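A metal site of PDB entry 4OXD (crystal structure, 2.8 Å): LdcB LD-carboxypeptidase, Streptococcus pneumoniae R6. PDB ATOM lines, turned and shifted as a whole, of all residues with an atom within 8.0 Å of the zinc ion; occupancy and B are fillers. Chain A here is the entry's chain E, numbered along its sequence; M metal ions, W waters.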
ATOM      1  N   SER A  66      19.366 -31.622  -2.054  1.00  0.00           N
ATOM      2  CA  SER A  66      18.419 -32.730  -2.248  1.00  0.00           C
ATOM      3  C   SER A  66      17.798 -32.608  -3.631  1.00  0.00           C
ATOM      4  O   SER A  66      16.805 -31.892  -3.817  1.00  0.00           O
ATOM      5  CB  SER A  66      17.317 -32.732  -1.179  1.00  0.00           C
ATOM      6  OG  SER A  66      16.598 -33.951  -1.199  1.00  0.00           O
ATOM      7  N   GLY A  67      18.380 -33.307  -4.597  1.00  0.00           N
ATOM      8  CA  GLY A  67      17.889 -33.268  -5.974  1.00  0.00           C
ATOM      9  C   GLY A  67      16.916 -34.383  -6.257  1.00  0.00           C
ATOM     10  O   GLY A  67      15.787 -34.384  -5.757  1.00  0.00           O
ATOM     11  N   ARG A  69      15.047 -37.951  -6.313  1.00  0.00           N
ATOM     12  CA  ARG A  69      14.708 -39.099  -5.479  1.00  0.00           C
ATOM     13  C   ARG A  69      13.772 -40.018  -6.257  1.00  0.00           C
ATOM     14  O   ARG A  69      12.644 -39.629  -6.597  1.00  0.00           O
ATOM     15  CB  ARG A  69      14.045 -38.658  -4.171  1.00  0.00           C
ATOM     16  CG  ARG A  69      14.980 -37.955  -3.210  1.00  0.00           C
ATOM     17  CD  ARG A  69      14.515 -38.120  -1.767  1.00  0.00           C
ATOM     18  NE  ARG A  69      13.115 -37.722  -1.574  1.00  0.00           N
ATOM     19  CZ  ARG A  69      12.701 -36.465  -1.407  1.00  0.00           C
ATOM     20  NH1 ARG A  69      11.395 -36.224  -1.235  1.00  0.00           N
ATOM     21  NH2 ARG A  69      13.557 -35.448  -1.392  1.00  0.00           N
ATOM     22  N   SER A 100       5.936 -37.027  -5.344  1.00  0.00           N
ATOM     23  CA  SER A 100       7.024 -36.082  -5.080  1.00  0.00           C
ATOM     24  C   SER A 100       7.506 -35.435  -6.369  1.00  0.00           C
ATOM     25  O   SER A 100       7.567 -36.085  -7.410  1.00  0.00           O
ATOM     26  CB  SER A 100       8.189 -36.787  -4.388  1.00  0.00           C
ATOM     27  OG  SER A 100       9.296 -35.921  -4.218  1.00  0.00           O
ATOM     28  N   GLU A 101       7.866 -34.151  -6.287  1.00  0.00           N
ATOM     29  CA  GLU A 101       8.372 -33.437  -7.460  1.00  0.00           C
ATOM     30  C   GLU A 101       9.842 -33.767  -7.716  1.00  0.00           C
ATOM     31  O   GLU A 101      10.347 -33.537  -8.818  1.00  0.00           O
ATOM     32  CB  GLU A 101       8.194 -31.925  -7.283  1.00  0.00           C
ATOM     33  CG  GLU A 101       8.363 -31.146  -8.593  1.00  0.00           C
ATOM     34  CD  GLU A 101       7.992 -29.685  -8.459  1.00  0.00           C
ATOM     35  OE1 GLU A 101       8.423 -29.040  -7.484  1.00  0.00           O
ATOM     36  OE2 GLU A 101       7.283 -29.169  -9.355  1.00  0.00           O
ATOM     37  N   HIS A 102      10.523 -34.313  -6.704  1.00  0.00           N
ATOM     38  CA  HIS A 102      11.926 -34.705  -6.830  1.00  0.00           C
ATOM     39  C   HIS A 102      12.144 -35.842  -7.834  1.00  0.00           C
ATOM     40  O   HIS A 102      13.243 -35.982  -8.378  1.00  0.00           O
ATOM     41  CB  HIS A 102      12.505 -35.119  -5.474  1.00  0.00           C
ATOM     42  CG  HIS A 102      12.632 -33.977  -4.509  1.00  0.00           C
ATOM     43  ND1 HIS A 102      13.738 -33.170  -4.459  1.00  0.00           N
ATOM     44  CD2 HIS A 102      11.796 -33.528  -3.545  1.00  0.00           C
ATOM     45  CE1 HIS A 102      13.592 -32.265  -3.498  1.00  0.00           C
ATOM     46  NE2 HIS A 102      12.393 -32.434  -2.967  1.00  0.00           N
ATOM     47  N   ALA A 107      13.284 -30.563  -9.480  1.00  0.00           N
ATOM     48  CA  ALA A 107      13.151 -29.957  -8.156  1.00  0.00           C
ATOM     49  C   ALA A 107      14.420 -30.177  -7.327  1.00  0.00           C
ATOM     50  O   ALA A 107      14.977 -31.271  -7.321  1.00  0.00           O
ATOM     51  CB  ALA A 107      11.947 -30.528  -7.435  1.00  0.00           C
ATOM     52  N   PHE A 108      14.876 -29.126  -6.637  1.00  0.00           N
ATOM     53  CA  PHE A 108      16.091 -29.184  -5.824  1.00  0.00           C
ATOM     54  C   PHE A 108      15.921 -28.399  -4.516  1.00  0.00           C
ATOM     55  O   PHE A 108      15.447 -27.262  -4.543  1.00  0.00           O
ATOM     56  CB  PHE A 108      17.287 -28.602  -6.588  1.00  0.00           C
ATOM     57  CG  PHE A 108      17.558 -29.280  -7.900  1.00  0.00           C
ATOM     58  CD1 PHE A 108      18.401 -30.388  -7.967  1.00  0.00           C
ATOM     59  CD2 PHE A 108      16.990 -28.813  -9.072  1.00  0.00           C
ATOM     60  CE1 PHE A 108      18.661 -31.018  -9.174  1.00  0.00           C
ATOM     61  CE2 PHE A 108      17.245 -29.445 -10.288  1.00  0.00           C
ATOM     62  CZ  PHE A 108      18.076 -30.546 -10.337  1.00  0.00           C
ATOM     63  N   ASP A 109      16.304 -29.003  -3.391  1.00  0.00           N
ATOM     64  CA  ASP A 109      16.273 -28.326  -2.092  1.00  0.00           C
ATOM     65  C   ASP A 109      17.629 -27.730  -1.748  1.00  0.00           C
ATOM     66  O   ASP A 109      18.641 -28.433  -1.750  1.00  0.00           O
ATOM     67  CB  ASP A 109      15.862 -29.288  -0.974  1.00  0.00           C
ATOM     68  CG  ASP A 109      14.494 -29.901  -1.180  1.00  0.00           C
ATOM     69  OD1 ASP A 109      13.674 -29.342  -1.935  1.00  0.00           O
ATOM     70  OD2 ASP A 109      14.228 -30.958  -0.566  1.00  0.00           O
ATOM     71  N   VAL A 110      17.630 -26.440  -1.421  1.00  0.00           N
ATOM     72  CA  VAL A 110      18.831 -25.739  -0.966  1.00  0.00           C
ATOM     73  C   VAL A 110      19.093 -26.068   0.518  1.00  0.00           C
ATOM     74  O   VAL A 110      18.140 -26.274   1.283  1.00  0.00           O
ATOM     75  CB  VAL A 110      18.690 -24.223  -1.220  1.00  0.00           C
ATOM     76  CG1 VAL A 110      19.616 -23.403  -0.340  1.00  0.00           C
ATOM     77  CG2 VAL A 110      18.961 -23.917  -2.686  1.00  0.00           C
ATOM     78  N   ARG A 139       8.601 -23.051  -5.428  1.00  0.00           N
ATOM     79  CA  ARG A 139       7.393 -23.818  -5.729  1.00  0.00           C
ATOM     80  C   ARG A 139       6.286 -23.610  -4.699  1.00  0.00           C
ATOM     81  O   ARG A 139       5.166 -23.224  -5.043  1.00  0.00           O
ATOM     82  CB  ARG A 139       7.743 -25.298  -5.826  1.00  0.00           C
ATOM     83  CG  ARG A 139       6.642 -26.188  -6.382  1.00  0.00           C
ATOM     84  CD  ARG A 139       6.538 -26.069  -7.893  1.00  0.00           C
ATOM     85  NE  ARG A 139       5.589 -27.028  -8.459  1.00  0.00           N
ATOM     86  CZ  ARG A 139       4.264 -26.902  -8.387  1.00  0.00           C
ATOM     87  NH1 ARG A 139       3.495 -27.844  -8.933  1.00  0.00           N
ATOM     88  NH2 ARG A 139       3.703 -25.859  -7.788  1.00  0.00           N
ATOM     89  N   TYR A 140       6.586 -23.884  -3.433  1.00  0.00           N
ATOM     90  CA  TYR A 140       5.585 -23.830  -2.361  1.00  0.00           C
ATOM     91  C   TYR A 140       5.631 -22.482  -1.636  1.00  0.00           C
ATOM     92  O   TYR A 140       6.230 -22.344  -0.570  1.00  0.00           O
ATOM     93  CB  TYR A 140       5.781 -25.004  -1.394  1.00  0.00           C
ATOM     94  CG  TYR A 140       5.905 -26.338  -2.116  1.00  0.00           C
ATOM     95  CD1 TYR A 140       4.910 -26.751  -3.002  1.00  0.00           C
ATOM     96  CD2 TYR A 140       7.011 -27.164  -1.921  1.00  0.00           C
ATOM     97  CE1 TYR A 140       5.016 -27.965  -3.672  1.00  0.00           C
ATOM     98  CE2 TYR A 140       7.109 -28.376  -2.587  1.00  0.00           C
ATOM     99  CZ  TYR A 140       6.113 -28.766  -3.464  1.00  0.00           C
ATOM    100  OH  TYR A 140       6.198 -29.966  -4.136  1.00  0.00           O
ATOM    101  N   TYR A 150       1.031 -28.665  -0.654  1.00  0.00           N
ATOM    102  CA  TYR A 150       2.129 -28.793   0.309  1.00  0.00           C
ATOM    103  C   TYR A 150       2.203 -27.549   1.184  1.00  0.00           C
ATOM    104  O   TYR A 150       1.879 -26.446   0.736  1.00  0.00           O
ATOM    105  CB  TYR A 150       3.460 -28.946  -0.428  1.00  0.00           C
ATOM    106  CG  TYR A 150       3.593 -30.218  -1.234  1.00  0.00           C
ATOM    107  CD1 TYR A 150       3.025 -30.326  -2.498  1.00  0.00           C
ATOM    108  CD2 TYR A 150       4.295 -31.298  -0.731  1.00  0.00           C
ATOM    109  CE1 TYR A 150       3.146 -31.495  -3.230  1.00  0.00           C
ATOM    110  CE2 TYR A 150       4.430 -32.468  -1.459  1.00  0.00           C
ATOM    111  CZ  TYR A 150       3.852 -32.561  -2.707  1.00  0.00           C
ATOM    112  OH  TYR A 150       3.980 -33.719  -3.433  1.00  0.00           O
ATOM    113  N   GLU A 153       7.448 -23.948   1.904  1.00  0.00           N
ATOM    114  CA  GLU A 153       8.859 -24.333   1.983  1.00  0.00           C
ATOM    115  C   GLU A 153       9.702 -23.242   1.306  1.00  0.00           C
ATOM    116  O   GLU A 153       9.435 -22.873   0.158  1.00  0.00           O
ATOM    117  CB  GLU A 153       9.083 -25.702   1.313  1.00  0.00           C
ATOM    118  CG  GLU A 153      10.464 -26.311   1.524  1.00  0.00           C
ATOM    119  CD  GLU A 153      10.675 -26.836   2.938  1.00  0.00           C
ATOM    120  OE1 GLU A 153      11.647 -26.410   3.602  1.00  0.00           O
ATOM    121  OE2 GLU A 153       9.868 -27.684   3.395  1.00  0.00           O
ATOM    122  N   TRP A 155      13.064 -23.248   0.650  1.00  0.00           N
ATOM    123  CA  TRP A 155      14.246 -23.682  -0.099  1.00  0.00           C
ATOM    124  C   TRP A 155      13.998 -24.738  -1.180  1.00  0.00           C
ATOM    125  O   TRP A 155      14.939 -25.156  -1.860  1.00  0.00           O
ATOM    126  CB  TRP A 155      15.318 -24.142   0.892  1.00  0.00           C
ATOM    127  CG  TRP A 155      15.662 -23.063   1.878  1.00  0.00           C
ATOM    128  CD1 TRP A 155      16.310 -21.889   1.619  1.00  0.00           C
ATOM    129  CD2 TRP A 155      15.337 -23.041   3.282  1.00  0.00           C
ATOM    130  NE1 TRP A 155      16.428 -21.140   2.763  1.00  0.00           N
ATOM    131  CE2 TRP A 155      15.844 -21.831   3.802  1.00  0.00           C
ATOM    132  CE3 TRP A 155      14.690 -23.932   4.142  1.00  0.00           C
ATOM    133  CZ2 TRP A 155      15.716 -21.482   5.148  1.00  0.00           C
ATOM    134  CZ3 TRP A 155      14.557 -23.584   5.480  1.00  0.00           C
ATOM    135  CH2 TRP A 155      15.073 -22.362   5.969  1.00  0.00           C
ATOM    136  N   HIS A 156      12.749 -25.147  -1.368  1.00  0.00           N
ATOM    137  CA  HIS A 156      12.383 -26.016  -2.488  1.00  0.00           C
ATOM    138  C   HIS A 156      12.282 -25.174  -3.767  1.00  0.00           C
ATOM    139  O   HIS A 156      11.464 -24.254  -3.852  1.00  0.00           O
ATOM    140  CB  HIS A 156      11.053 -26.729  -2.222  1.00  0.00           C
ATOM    141  CG  HIS A 156      10.673 -27.716  -3.282  1.00  0.00           C
ATOM    142  ND1 HIS A 156      10.721 -29.085  -3.088  1.00  0.00           N
ATOM    143  CD2 HIS A 156      10.272 -27.545  -4.568  1.00  0.00           C
ATOM    144  CE1 HIS A 156      10.331 -29.706  -4.196  1.00  0.00           C
ATOM    145  NE2 HIS A 156      10.064 -28.788  -5.107  1.00  0.00           N
ATOM    146  N   LEU A 157      13.115 -25.504  -4.758  1.00  0.00           N
ATOM    147  CA  LEU A 157      13.168 -24.767  -6.019  1.00  0.00           C
ATOM    148  C   LEU A 157      12.831 -25.675  -7.197  1.00  0.00           C
ATOM    149  O   LEU A 157      13.324 -26.807  -7.265  1.00  0.00           O
ATOM    150  CB  LEU A 157      14.574 -24.178  -6.229  1.00  0.00           C
ATOM    151  CG  LEU A 157      15.147 -23.287  -5.129  1.00  0.00           C
ATOM    152  CD1 LEU A 157      16.551 -22.828  -5.530  1.00  0.00           C
ATOM    153  CD2 LEU A 157      14.263 -22.088  -4.841  1.00  0.00           C
ATOM    154  N   ARG A 158      12.008 -25.177  -8.118  1.00  0.00           N
ATOM    155  CA  ARG A 158      11.604 -25.913  -9.317  1.00  0.00           C
ATOM    156  C   ARG A 158      12.105 -25.219 -10.577  1.00  0.00           C
ATOM    157  O   ARG A 158      11.791 -24.044 -10.808  1.00  0.00           O
ATOM    158  CB  ARG A 158      10.076 -26.044  -9.370  1.00  0.00           C
ATOM    159  CG  ARG A 158       9.511 -26.478 -10.729  1.00  0.00           C
ATOM    160  CD  ARG A 158      10.036 -27.834 -11.180  1.00  0.00           C
ATOM    161  NE  ARG A 158       9.631 -28.161 -12.543  1.00  0.00           N
ATOM    162  CZ  ARG A 158       8.459 -28.694 -12.887  1.00  0.00           C
ATOM    163  NH1 ARG A 158       7.526 -28.964 -11.984  1.00  0.00           N
ATOM    164  NH2 ARG A 158       8.215 -28.945 -14.168  1.00  0.00           N
HETATM  165 ZN    ZN M   1      12.081 -30.474  -2.331  1.00  0.00          ZN
HETATM  166  O   HOH W   1      11.006 -30.146  -0.659  1.00  0.00           O
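N of Asp 109 is in hydrogen-bond range of O of Ser 66, at 3.0 Å.
The backbone NH (N) of Arg 139 is in hydrogen-bond range of the backbone carbonyl oxygen (O) of His 156 (3.5 Å).
The backbone carbonyl oxygen (O) of Gly 67 is in hydrogen-bond range of a ring nitrogen (ND1) of His 102.
A ring nitrogen (ND1) of His 102 sits close to the backbone carbonyl oxygen (O) of Ser 66.
The backbone NH (N) of His 102 is in hydrogen-bond range of the side-chain hydroxyl (OG) of Ser 100 (3.2 Å).
NE2 of His 156 lies within hydrogen-bond range of OE1 of Glu 101, at 2.9 Å.
The backbone carbonyl oxygen (O) of His 102 is in hydrogen-bond range of the backbone NH (N) of Arg 69 (3.4 Å).
The nearest printed residue that does not touch the zinc ion is Phe 108 (4.9 Å).
The zinc ion is bound by the side-chain carboxylate of Asp 109 (2.0 Å), water W1 (2.0 Å), a ring nitrogen (NE2) of His 102 (2.1 Å) and a ring nitrogen (ND1) of His 156 (2.1 Å).
Slightly farther from the zinc ion lies OD2 of Asp 109 (2.8 Å).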
